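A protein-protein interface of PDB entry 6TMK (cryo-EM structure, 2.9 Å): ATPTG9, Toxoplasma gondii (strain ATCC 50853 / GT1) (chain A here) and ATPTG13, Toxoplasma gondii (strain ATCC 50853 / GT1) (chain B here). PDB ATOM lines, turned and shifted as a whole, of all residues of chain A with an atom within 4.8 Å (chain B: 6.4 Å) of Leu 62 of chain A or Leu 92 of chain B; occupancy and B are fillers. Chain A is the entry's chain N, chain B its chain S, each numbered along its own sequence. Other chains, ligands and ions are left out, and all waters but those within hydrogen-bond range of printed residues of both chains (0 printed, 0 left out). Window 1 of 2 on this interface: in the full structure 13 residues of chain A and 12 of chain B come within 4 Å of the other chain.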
ATOM      1  N   GLU A  58      13.647  -2.140 -11.706  1.00  0.00           N
ATOM      2  CA  GLU A  58      14.024  -1.111 -10.745  1.00  0.00           C
ATOM      3  C   GLU A  58      15.273  -1.518  -9.976  1.00  0.00           C
ATOM      4  O   GLU A  58      16.204  -0.718  -9.813  1.00  0.00           O
ATOM      5  CB  GLU A  58      12.863  -0.847  -9.792  1.00  0.00           C
ATOM      6  CG  GLU A  58      11.722  -0.070 -10.413  1.00  0.00           C
ATOM      7  CD  GLU A  58      10.812  -0.938 -11.255  1.00  0.00           C
ATOM      8  OE1 GLU A  58      11.187  -2.094 -11.536  1.00  0.00           O
ATOM      9  OE2 GLU A  58       9.720  -0.465 -11.635  1.00  0.00           O
ATOM     10  N   GLY A  59      15.322  -2.768  -9.513  1.00  0.00           N
ATOM     11  CA  GLY A  59      16.511  -3.237  -8.824  1.00  0.00           C
ATOM     12  C   GLY A  59      17.744  -3.194  -9.703  1.00  0.00           C
ATOM     13  O   GLY A  59      18.818  -2.764  -9.269  1.00  0.00           O
ATOM     14  N   ILE A  60      17.606  -3.630 -10.954  1.00  0.00           N
ATOM     15  CA  ILE A  60      18.747  -3.651 -11.861  1.00  0.00           C
ATOM     16  C   ILE A  60      19.226  -2.237 -12.152  1.00  0.00           C
ATOM     17  O   ILE A  60      20.433  -1.967 -12.170  1.00  0.00           O
ATOM     18  CB  ILE A  60      18.377  -4.404 -13.149  1.00  0.00           C
ATOM     19  CG1 ILE A  60      18.176  -5.888 -12.855  1.00  0.00           C
ATOM     20  CG2 ILE A  60      19.448  -4.216 -14.195  1.00  0.00           C
ATOM     21  CD1 ILE A  60      19.409  -6.591 -12.337  1.00  0.00           C
ATOM     22  N   ASN A  61      18.296  -1.314 -12.392  1.00  0.00           N
ATOM     23  CA  ASN A  61      18.682   0.062 -12.671  1.00  0.00           C
ATOM     24  C   ASN A  61      19.384   0.677 -11.472  1.00  0.00           C
ATOM     25  O   ASN A  61      20.377   1.396 -11.628  1.00  0.00           O
ATOM     26  CB  ASN A  61      17.452   0.878 -13.055  1.00  0.00           C
ATOM     27  CG  ASN A  61      16.928   0.524 -14.426  1.00  0.00           C
ATOM     28  OD1 ASN A  61      17.685   0.129 -15.311  1.00  0.00           O
ATOM     29  ND2 ASN A  61      15.623   0.663 -14.611  1.00  0.00           N
ATOM     30  N   LEU A  62      18.887   0.406 -10.266  1.00  0.00           N
ATOM     31  CA  LEU A  62      19.531   0.928  -9.069  1.00  0.00           C
ATOM     32  C   LEU A  62      20.946   0.388  -8.926  1.00  0.00           C
ATOM     33  O   LEU A  62      21.890   1.139  -8.643  1.00  0.00           O
ATOM     34  CB  LEU A  62      18.700   0.566  -7.842  1.00  0.00           C
ATOM     35  CG  LEU A  62      19.233   1.065  -6.503  1.00  0.00           C
ATOM     36  CD1 LEU A  62      19.236   2.564  -6.458  1.00  0.00           C
ATOM     37  CD2 LEU A  62      18.411   0.505  -5.386  1.00  0.00           C
ATOM     38  N   MET A  63      21.109  -0.923  -9.100  1.00  0.00           N
ATOM     39  CA  MET A  63      22.431  -1.524  -8.987  1.00  0.00           C
ATOM     40  C   MET A  63      23.390  -0.939 -10.012  1.00  0.00           C
ATOM     41  O   MET A  63      24.551  -0.655  -9.697  1.00  0.00           O
ATOM     42  CB  MET A  63      22.327  -3.032  -9.168  1.00  0.00           C
ATOM     43  CG  MET A  63      21.769  -3.769  -7.981  1.00  0.00           C
ATOM     44  SD  MET A  63      21.137  -5.379  -8.468  1.00  0.00           S
ATOM     45  CE  MET A  63      21.433  -6.304  -6.975  1.00  0.00           C
ATOM     46  N   LYS A  64      22.928  -0.757 -11.249  1.00  0.00           N
ATOM     47  CA  LYS A  64      23.785  -0.180 -12.277  1.00  0.00           C
ATOM     48  C   LYS A  64      24.148   1.262 -11.952  1.00  0.00           C
ATOM     49  O   LYS A  64      25.298   1.676 -12.140  1.00  0.00           O
ATOM     50  CB  LYS A  64      23.095  -0.258 -13.637  1.00  0.00           C
ATOM     51  CG  LYS A  64      23.105  -1.640 -14.254  1.00  0.00           C
ATOM     52  CD  LYS A  64      22.186  -1.722 -15.455  1.00  0.00           C
ATOM     53  CE  LYS A  64      22.202  -3.114 -16.064  1.00  0.00           C
ATOM     54  NZ  LYS A  64      21.096  -3.324 -17.036  1.00  0.00           N
ATOM     55  N   CYS A  65      23.185   2.039 -11.461  1.00  0.00           N
ATOM     56  CA  CYS A  65      23.429   3.455 -11.219  1.00  0.00           C
ATOM     57  C   CYS A  65      24.387   3.673 -10.056  1.00  0.00           C
ATOM     58  O   CYS A  65      25.264   4.540 -10.127  1.00  0.00           O
ATOM     59  CB  CYS A  65      22.106   4.173 -10.965  1.00  0.00           C
ATOM     60  SG  CYS A  65      21.129   4.467 -12.456  1.00  0.00           S
ATOM     61  N   THR A  66      24.244   2.903  -8.976  1.00  0.00           N
ATOM     62  CA  THR A  66      25.008   3.210  -7.772  1.00  0.00           C
ATOM     63  C   THR A  66      26.505   3.002  -7.953  1.00  0.00           C
ATOM     64  O   THR A  66      27.286   3.501  -7.136  1.00  0.00           O
ATOM     65  CB  THR A  66      24.522   2.379  -6.593  1.00  0.00           C
ATOM     66  OG1 THR A  66      24.501   0.992  -6.943  1.00  0.00           O
ATOM     67  CG2 THR A  66      23.147   2.827  -6.186  1.00  0.00           C
ATOM     68  N   CYS A  74      21.249   8.999  -7.469  1.00  0.00           N
ATOM     69  CA  CYS A  74      20.344   7.882  -7.727  1.00  0.00           C
ATOM     70  C   CYS A  74      19.096   7.940  -6.856  1.00  0.00           C
ATOM     71  O   CYS A  74      18.499   6.907  -6.539  1.00  0.00           O
ATOM     72  CB  CYS A  74      21.058   6.543  -7.539  1.00  0.00           C
ATOM     73  SG  CYS A  74      22.739   6.504  -8.178  1.00  0.00           S
ATOM     74  N   GLU A  77      15.961   6.526  -8.520  1.00  0.00           N
ATOM     75  CA  GLU A  77      16.025   5.070  -8.525  1.00  0.00           C
ATOM     76  C   GLU A  77      15.676   4.502  -7.157  1.00  0.00           C
ATOM     77  O   GLU A  77      14.927   3.522  -7.051  1.00  0.00           O
ATOM     78  CB  GLU A  77      17.418   4.620  -8.950  1.00  0.00           C
ATOM     79  CG  GLU A  77      17.668   4.678 -10.439  1.00  0.00           C
ATOM     80  CD  GLU A  77      17.842   6.091 -10.951  1.00  0.00           C
ATOM     81  OE1 GLU A  77      18.488   6.901 -10.256  1.00  0.00           O
ATOM     82  OE2 GLU A  77      17.334   6.395 -12.050  1.00  0.00           O
ATOM     83  N   PHE A  78      16.216   5.102  -6.097  1.00  0.00           N
ATOM     84  CA  PHE A  78      15.932   4.626  -4.749  1.00  0.00           C
ATOM     85  C   PHE A  78      14.442   4.693  -4.448  1.00  0.00           C
ATOM     86  O   PHE A  78      13.842   3.715  -3.984  1.00  0.00           O
ATOM     87  CB  PHE A  78      16.713   5.456  -3.739  1.00  0.00           C
ATOM     88  CG  PHE A  78      18.100   4.971  -3.497  1.00  0.00           C
ATOM     89  CD1 PHE A  78      18.326   3.791  -2.830  1.00  0.00           C
ATOM     90  CD2 PHE A  78      19.183   5.699  -3.931  1.00  0.00           C
ATOM     91  CE1 PHE A  78      19.597   3.351  -2.605  1.00  0.00           C
ATOM     92  CE2 PHE A  78      20.456   5.258  -3.708  1.00  0.00           C
ATOM     93  CZ  PHE A  78      20.662   4.083  -3.047  1.00  0.00           C
ATOM     94  N   MET A  81      12.405   2.117  -6.467  1.00  0.00           N
ATOM     95  CA  MET A  81      12.477   0.775  -5.903  1.00  0.00           C
ATOM     96  C   MET A  81      11.632   0.669  -4.642  1.00  0.00           C
ATOM     97  O   MET A  81      10.899  -0.312  -4.449  1.00  0.00           O
ATOM     98  CB  MET A  81      13.930   0.413  -5.613  1.00  0.00           C
ATOM     99  CG  MET A  81      14.141  -1.016  -5.169  1.00  0.00           C
ATOM    100  SD  MET A  81      13.642  -2.216  -6.411  1.00  0.00           S
ATOM    101  CE  MET A  81      13.416  -3.666  -5.388  1.00  0.00           C
ATOM    102  N   ARG A  82      11.722   1.677  -3.775  1.00  0.00           N
ATOM    103  CA  ARG A  82      10.955   1.661  -2.538  1.00  0.00           C
ATOM    104  C   ARG A  82       9.462   1.606  -2.814  1.00  0.00           C
ATOM    105  O   ARG A  82       8.716   0.932  -2.095  1.00  0.00           O
ATOM    106  CB  ARG A  82      11.295   2.895  -1.707  1.00  0.00           C
ATOM    107  CG  ARG A  82      10.658   2.914  -0.347  1.00  0.00           C
ATOM    108  CD  ARG A  82       9.432   3.790  -0.305  1.00  0.00           C
ATOM    109  NE  ARG A  82       8.883   3.871   1.039  1.00  0.00           N
ATOM    110  CZ  ARG A  82       8.256   2.873   1.646  1.00  0.00           C
ATOM    111  NH1 ARG A  82       8.094   1.711   1.037  1.00  0.00           N
ATOM    112  NH2 ARG A  82       7.796   3.039   2.870  1.00  0.00           N
ATOM    113  N   ASP B  87      23.949   5.509   3.253  1.00  0.00           N
ATOM    114  CA  ASP B  87      22.803   5.901   4.058  1.00  0.00           C
ATOM    115  C   ASP B  87      21.503   5.615   3.323  1.00  0.00           C
ATOM    116  O   ASP B  87      20.524   5.150   3.926  1.00  0.00           O
ATOM    117  CB  ASP B  87      22.911   7.378   4.422  1.00  0.00           C
ATOM    118  CG  ASP B  87      21.788   7.845   5.326  1.00  0.00           C
ATOM    119  OD1 ASP B  87      20.946   8.647   4.867  1.00  0.00           O
ATOM    120  OD2 ASP B  87      21.753   7.416   6.501  1.00  0.00           O
ATOM    121  N   ARG B  88      21.478   5.855   2.012  1.00  0.00           N
ATOM    122  CA  ARG B  88      20.263   5.580   1.254  1.00  0.00           C
ATOM    123  C   ARG B  88      19.984   4.085   1.151  1.00  0.00           C
ATOM    124  O   ARG B  88      18.818   3.673   1.163  1.00  0.00           O
ATOM    125  CB  ARG B  88      20.363   6.219  -0.119  1.00  0.00           C
ATOM    126  CG  ARG B  88      20.253   7.701  -0.059  1.00  0.00           C
ATOM    127  CD  ARG B  88      20.344   8.338  -1.398  1.00  0.00           C
ATOM    128  NE  ARG B  88      20.270   9.787  -1.302  1.00  0.00           N
ATOM    129  CZ  ARG B  88      20.356  10.605  -2.340  1.00  0.00           C
ATOM    130  NH1 ARG B  88      20.511  10.113  -3.553  1.00  0.00           N
ATOM    131  NH2 ARG B  88      20.279  11.909  -2.162  1.00  0.00           N
ATOM    132  N   TYR B  89      21.026   3.256   1.070  1.00  0.00           N
ATOM    133  CA  TYR B  89      20.815   1.812   1.061  1.00  0.00           C
ATOM    134  C   TYR B  89      20.272   1.326   2.396  1.00  0.00           C
ATOM    135  O   TYR B  89      19.428   0.426   2.438  1.00  0.00           O
ATOM    136  CB  TYR B  89      22.110   1.087   0.714  1.00  0.00           C
ATOM    137  CG  TYR B  89      22.286   0.821  -0.758  1.00  0.00           C
ATOM    138  CD1 TYR B  89      21.421  -0.017  -1.432  1.00  0.00           C
ATOM    139  CD2 TYR B  89      23.313   1.402  -1.471  1.00  0.00           C
ATOM    140  CE1 TYR B  89      21.572  -0.265  -2.768  1.00  0.00           C
ATOM    141  CE2 TYR B  89      23.470   1.158  -2.808  1.00  0.00           C
ATOM    142  CZ  TYR B  89      22.596   0.324  -3.453  1.00  0.00           C
ATOM    143  OH  TYR B  89      22.749   0.072  -4.793  1.00  0.00           O
ATOM    144  N   THR B  90      20.747   1.903   3.496  1.00  0.00           N
ATOM    145  CA  THR B  90      20.213   1.542   4.807  1.00  0.00           C
ATOM    146  C   THR B  90      18.735   1.906   4.901  1.00  0.00           C
ATOM    147  O   THR B  90      17.903   1.117   5.381  1.00  0.00           O
ATOM    148  CB  THR B  90      21.015   2.245   5.898  1.00  0.00           C
ATOM    149  OG1 THR B  90      22.403   1.935   5.749  1.00  0.00           O
ATOM    150  CG2 THR B  90      20.565   1.796   7.250  1.00  0.00           C
ATOM    151  N   TRP B  91      18.398   3.115   4.455  1.00  0.00           N
ATOM    152  CA  TRP B  91      17.006   3.535   4.367  1.00  0.00           C
ATOM    153  C   TRP B  91      16.169   2.523   3.591  1.00  0.00           C
ATOM    154  O   TRP B  91      15.106   2.084   4.053  1.00  0.00           O
ATOM    155  CB  TRP B  91      16.971   4.918   3.717  1.00  0.00           C
ATOM    156  CG  TRP B  91      15.631   5.471   3.430  1.00  0.00           C
ATOM    157  CD1 TRP B  91      14.828   6.147   4.285  1.00  0.00           C
ATOM    158  CD2 TRP B  91      14.943   5.425   2.181  1.00  0.00           C
ATOM    159  NE1 TRP B  91      13.671   6.514   3.655  1.00  0.00           N
ATOM    160  CE2 TRP B  91      13.718   6.081   2.358  1.00  0.00           C
ATOM    161  CE3 TRP B  91      15.240   4.883   0.932  1.00  0.00           C
ATOM    162  CZ2 TRP B  91      12.792   6.211   1.337  1.00  0.00           C
ATOM    163  CZ3 TRP B  91      14.325   5.013  -0.074  1.00  0.00           C
ATOM    164  CH2 TRP B  91      13.116   5.671   0.129  1.00  0.00           C
ATOM    165  N   LEU B  92      16.632   2.149   2.399  1.00  0.00           N
ATOM    166  CA  LEU B  92      15.893   1.209   1.566  1.00  0.00           C
ATOM    167  C   LEU B  92      15.727  -0.142   2.248  1.00  0.00           C
ATOM    168  O   LEU B  92      14.675  -0.779   2.131  1.00  0.00           O
ATOM    169  CB  LEU B  92      16.608   1.044   0.235  1.00  0.00           C
ATOM    170  CG  LEU B  92      15.948   0.126  -0.779  1.00  0.00           C
ATOM    171  CD1 LEU B  92      14.617   0.679  -1.193  1.00  0.00           C
ATOM    172  CD2 LEU B  92      16.852  -0.025  -1.954  1.00  0.00           C
ATOM    173  N   HIS B  93      16.764  -0.604   2.940  1.00  0.00           N
ATOM    174  CA  HIS B  93      16.687  -1.861   3.674  1.00  0.00           C
ATOM    175  C   HIS B  93      15.554  -1.826   4.689  1.00  0.00           C
ATOM    176  O   HIS B  93      14.719  -2.744   4.753  1.00  0.00           O
ATOM    177  CB  HIS B  93      18.032  -2.113   4.349  1.00  0.00           C
ATOM    178  CG  HIS B  93      18.120  -3.408   5.088  1.00  0.00           C
ATOM    179  ND1 HIS B  93      18.619  -3.494   6.369  1.00  0.00           N
ATOM    180  CD2 HIS B  93      17.798  -4.669   4.725  1.00  0.00           C
ATOM    181  CE1 HIS B  93      18.589  -4.752   6.765  1.00  0.00           C
ATOM    182  NE2 HIS B  93      18.097  -5.485   5.786  1.00  0.00           N
ATOM    183  N   GLU B  94      15.508  -0.765   5.488  1.00  0.00           N
ATOM    184  CA  GLU B  94      14.464  -0.656   6.500  1.00  0.00           C
ATOM    185  C   GLU B  94      13.080  -0.606   5.865  1.00  0.00           C
ATOM    186  O   GLU B  94      12.131  -1.236   6.356  1.00  0.00           O
ATOM    187  CB  GLU B  94      14.715   0.576   7.353  1.00  0.00           C
ATOM    188  CG  GLU B  94      15.818   0.386   8.348  1.00  0.00           C
ATOM    189  CD  GLU B  94      16.547   1.671   8.671  1.00  0.00           C
ATOM    190  OE1 GLU B  94      15.983   2.757   8.428  1.00  0.00           O
ATOM    191  OE2 GLU B  94      17.691   1.592   9.165  1.00  0.00           O
ATOM    192  N   ARG B  95      12.947   0.129   4.761  1.00  0.00           N
ATOM    193  CA  ARG B  95      11.644   0.239   4.117  1.00  0.00           C
ATOM    194  C   ARG B  95      11.202  -1.095   3.527  1.00  0.00           C
ATOM    195  O   ARG B  95      10.013  -1.432   3.558  1.00  0.00           O
ATOM    196  CB  ARG B  95      11.696   1.314   3.038  1.00  0.00           C
ATOM    197  CG  ARG B  95      12.076   2.678   3.549  1.00  0.00           C
ATOM    198  CD  ARG B  95      10.998   3.312   4.398  1.00  0.00           C
ATOM    199  NE  ARG B  95      11.010   2.865   5.787  1.00  0.00           N
ATOM    200  CZ  ARG B  95      11.972   3.145   6.657  1.00  0.00           C
ATOM    201  NH1 ARG B  95      11.891   2.702   7.899  1.00  0.00           N
ATOM    202  NH2 ARG B  95      13.016   3.861   6.289  1.00  0.00           N
ATOM    203  N   MET B  96      12.143  -1.873   2.997  1.00  0.00           N
ATOM    204  CA  MET B  96      11.802  -3.184   2.460  1.00  0.00           C
ATOM    205  C   MET B  96      11.356  -4.133   3.566  1.00  0.00           C
ATOM    206  O   MET B  96      10.431  -4.934   3.374  1.00  0.00           O
ATOM    207  CB  MET B  96      12.994  -3.751   1.701  1.00  0.00           C
ATOM    208  CG  MET B  96      13.262  -3.041   0.392  1.00  0.00           C
ATOM    209  SD  MET B  96      14.843  -3.455  -0.346  1.00  0.00           S
ATOM    210  CE  MET B  96      14.401  -4.953  -1.202  1.00  0.00           C
ATOM    211  N   LEU B  97      11.992  -4.051   4.733  1.00  0.00           N
ATOM    212  CA  LEU B  97      11.528  -4.847   5.865  1.00  0.00           C
ATOM    213  C   LEU B  97      10.110  -4.458   6.266  1.00  0.00           C
ATOM    214  O   LEU B  97       9.267  -5.325   6.544  1.00  0.00           O
ATOM    215  CB  LEU B  97      12.474  -4.684   7.047  1.00  0.00           C
ATOM    216  CG  LEU B  97      13.891  -5.210   6.858  1.00  0.00           C
ATOM    217  CD1 LEU B  97      14.720  -4.913   8.074  1.00  0.00           C
ATOM    218  CD2 LEU B  97      13.891  -6.680   6.570  1.00  0.00           C
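The side-chain hydroxyl (OG1) of Thr 66 of chain A is in hydrogen-bond range of the side-chain hydroxyl (OH) of Tyr 89 of chain B.
Among the printed residues, pairs that only touch across the chains: Arg 82 of chain A with Arg 95 of chain B (3.6 Å), Phe 78 of chain A with Arg 88 of chain B (3.6 Å), Arg 82 of chain A with Trp 91 of chain B (3.7 Å), Leu 62 of chain A with Leu 92 of chain B (3.8 Å) and Phe 78 of chain A with Tyr 89 of chain B (3.9 Å).
Cys 65 of chain A touches none of the printed residues of chain B. Of the printed residues of chain B, Phe 78 of chain A touches Arg 88 (3.6 Å) and Tyr 89 (3.9 Å). Printed residues of chain A within 4 Å of Arg 88 of chain B: Phe 78. Printed residues of chain A within 4 Å of Tyr 89 of chain B: Thr 66 and Phe 78. Printed residues of chain A within 4 Å of Trp 91 of chain B: Arg 82. Of the printed residues of chain A, Leu 92 of chain B touches Leu 62. His 93 of chain B touches none of the printed residues of chain A. Of the printed residues of chain A, Arg 95 of chain B touches Arg 82.
The backbone carbonyl oxygen of Leu 62 of chain A is in hydrogen-bond range of the side-chain hydroxyl of Thr 66 of chain A, 3.1 Å away. The backbone carbonyl oxygen (O) of Met 63 of chain A sits at hydrogen-bond distance from the side-chain hydroxyl (OG1) of Thr 66 of chain A, at 3.2 Å. The side-chain carboxylate (OE1) of Glu 94 of chain B is in salt-bridge range of the guanidinium group (NH2) of Arg 95 of chain B, 3.8 Å away.
Among the printed residues, no Asp or Glu carboxylate lies within 4 Å of a Lys or Arg side-chain nitrogen of the other chain.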
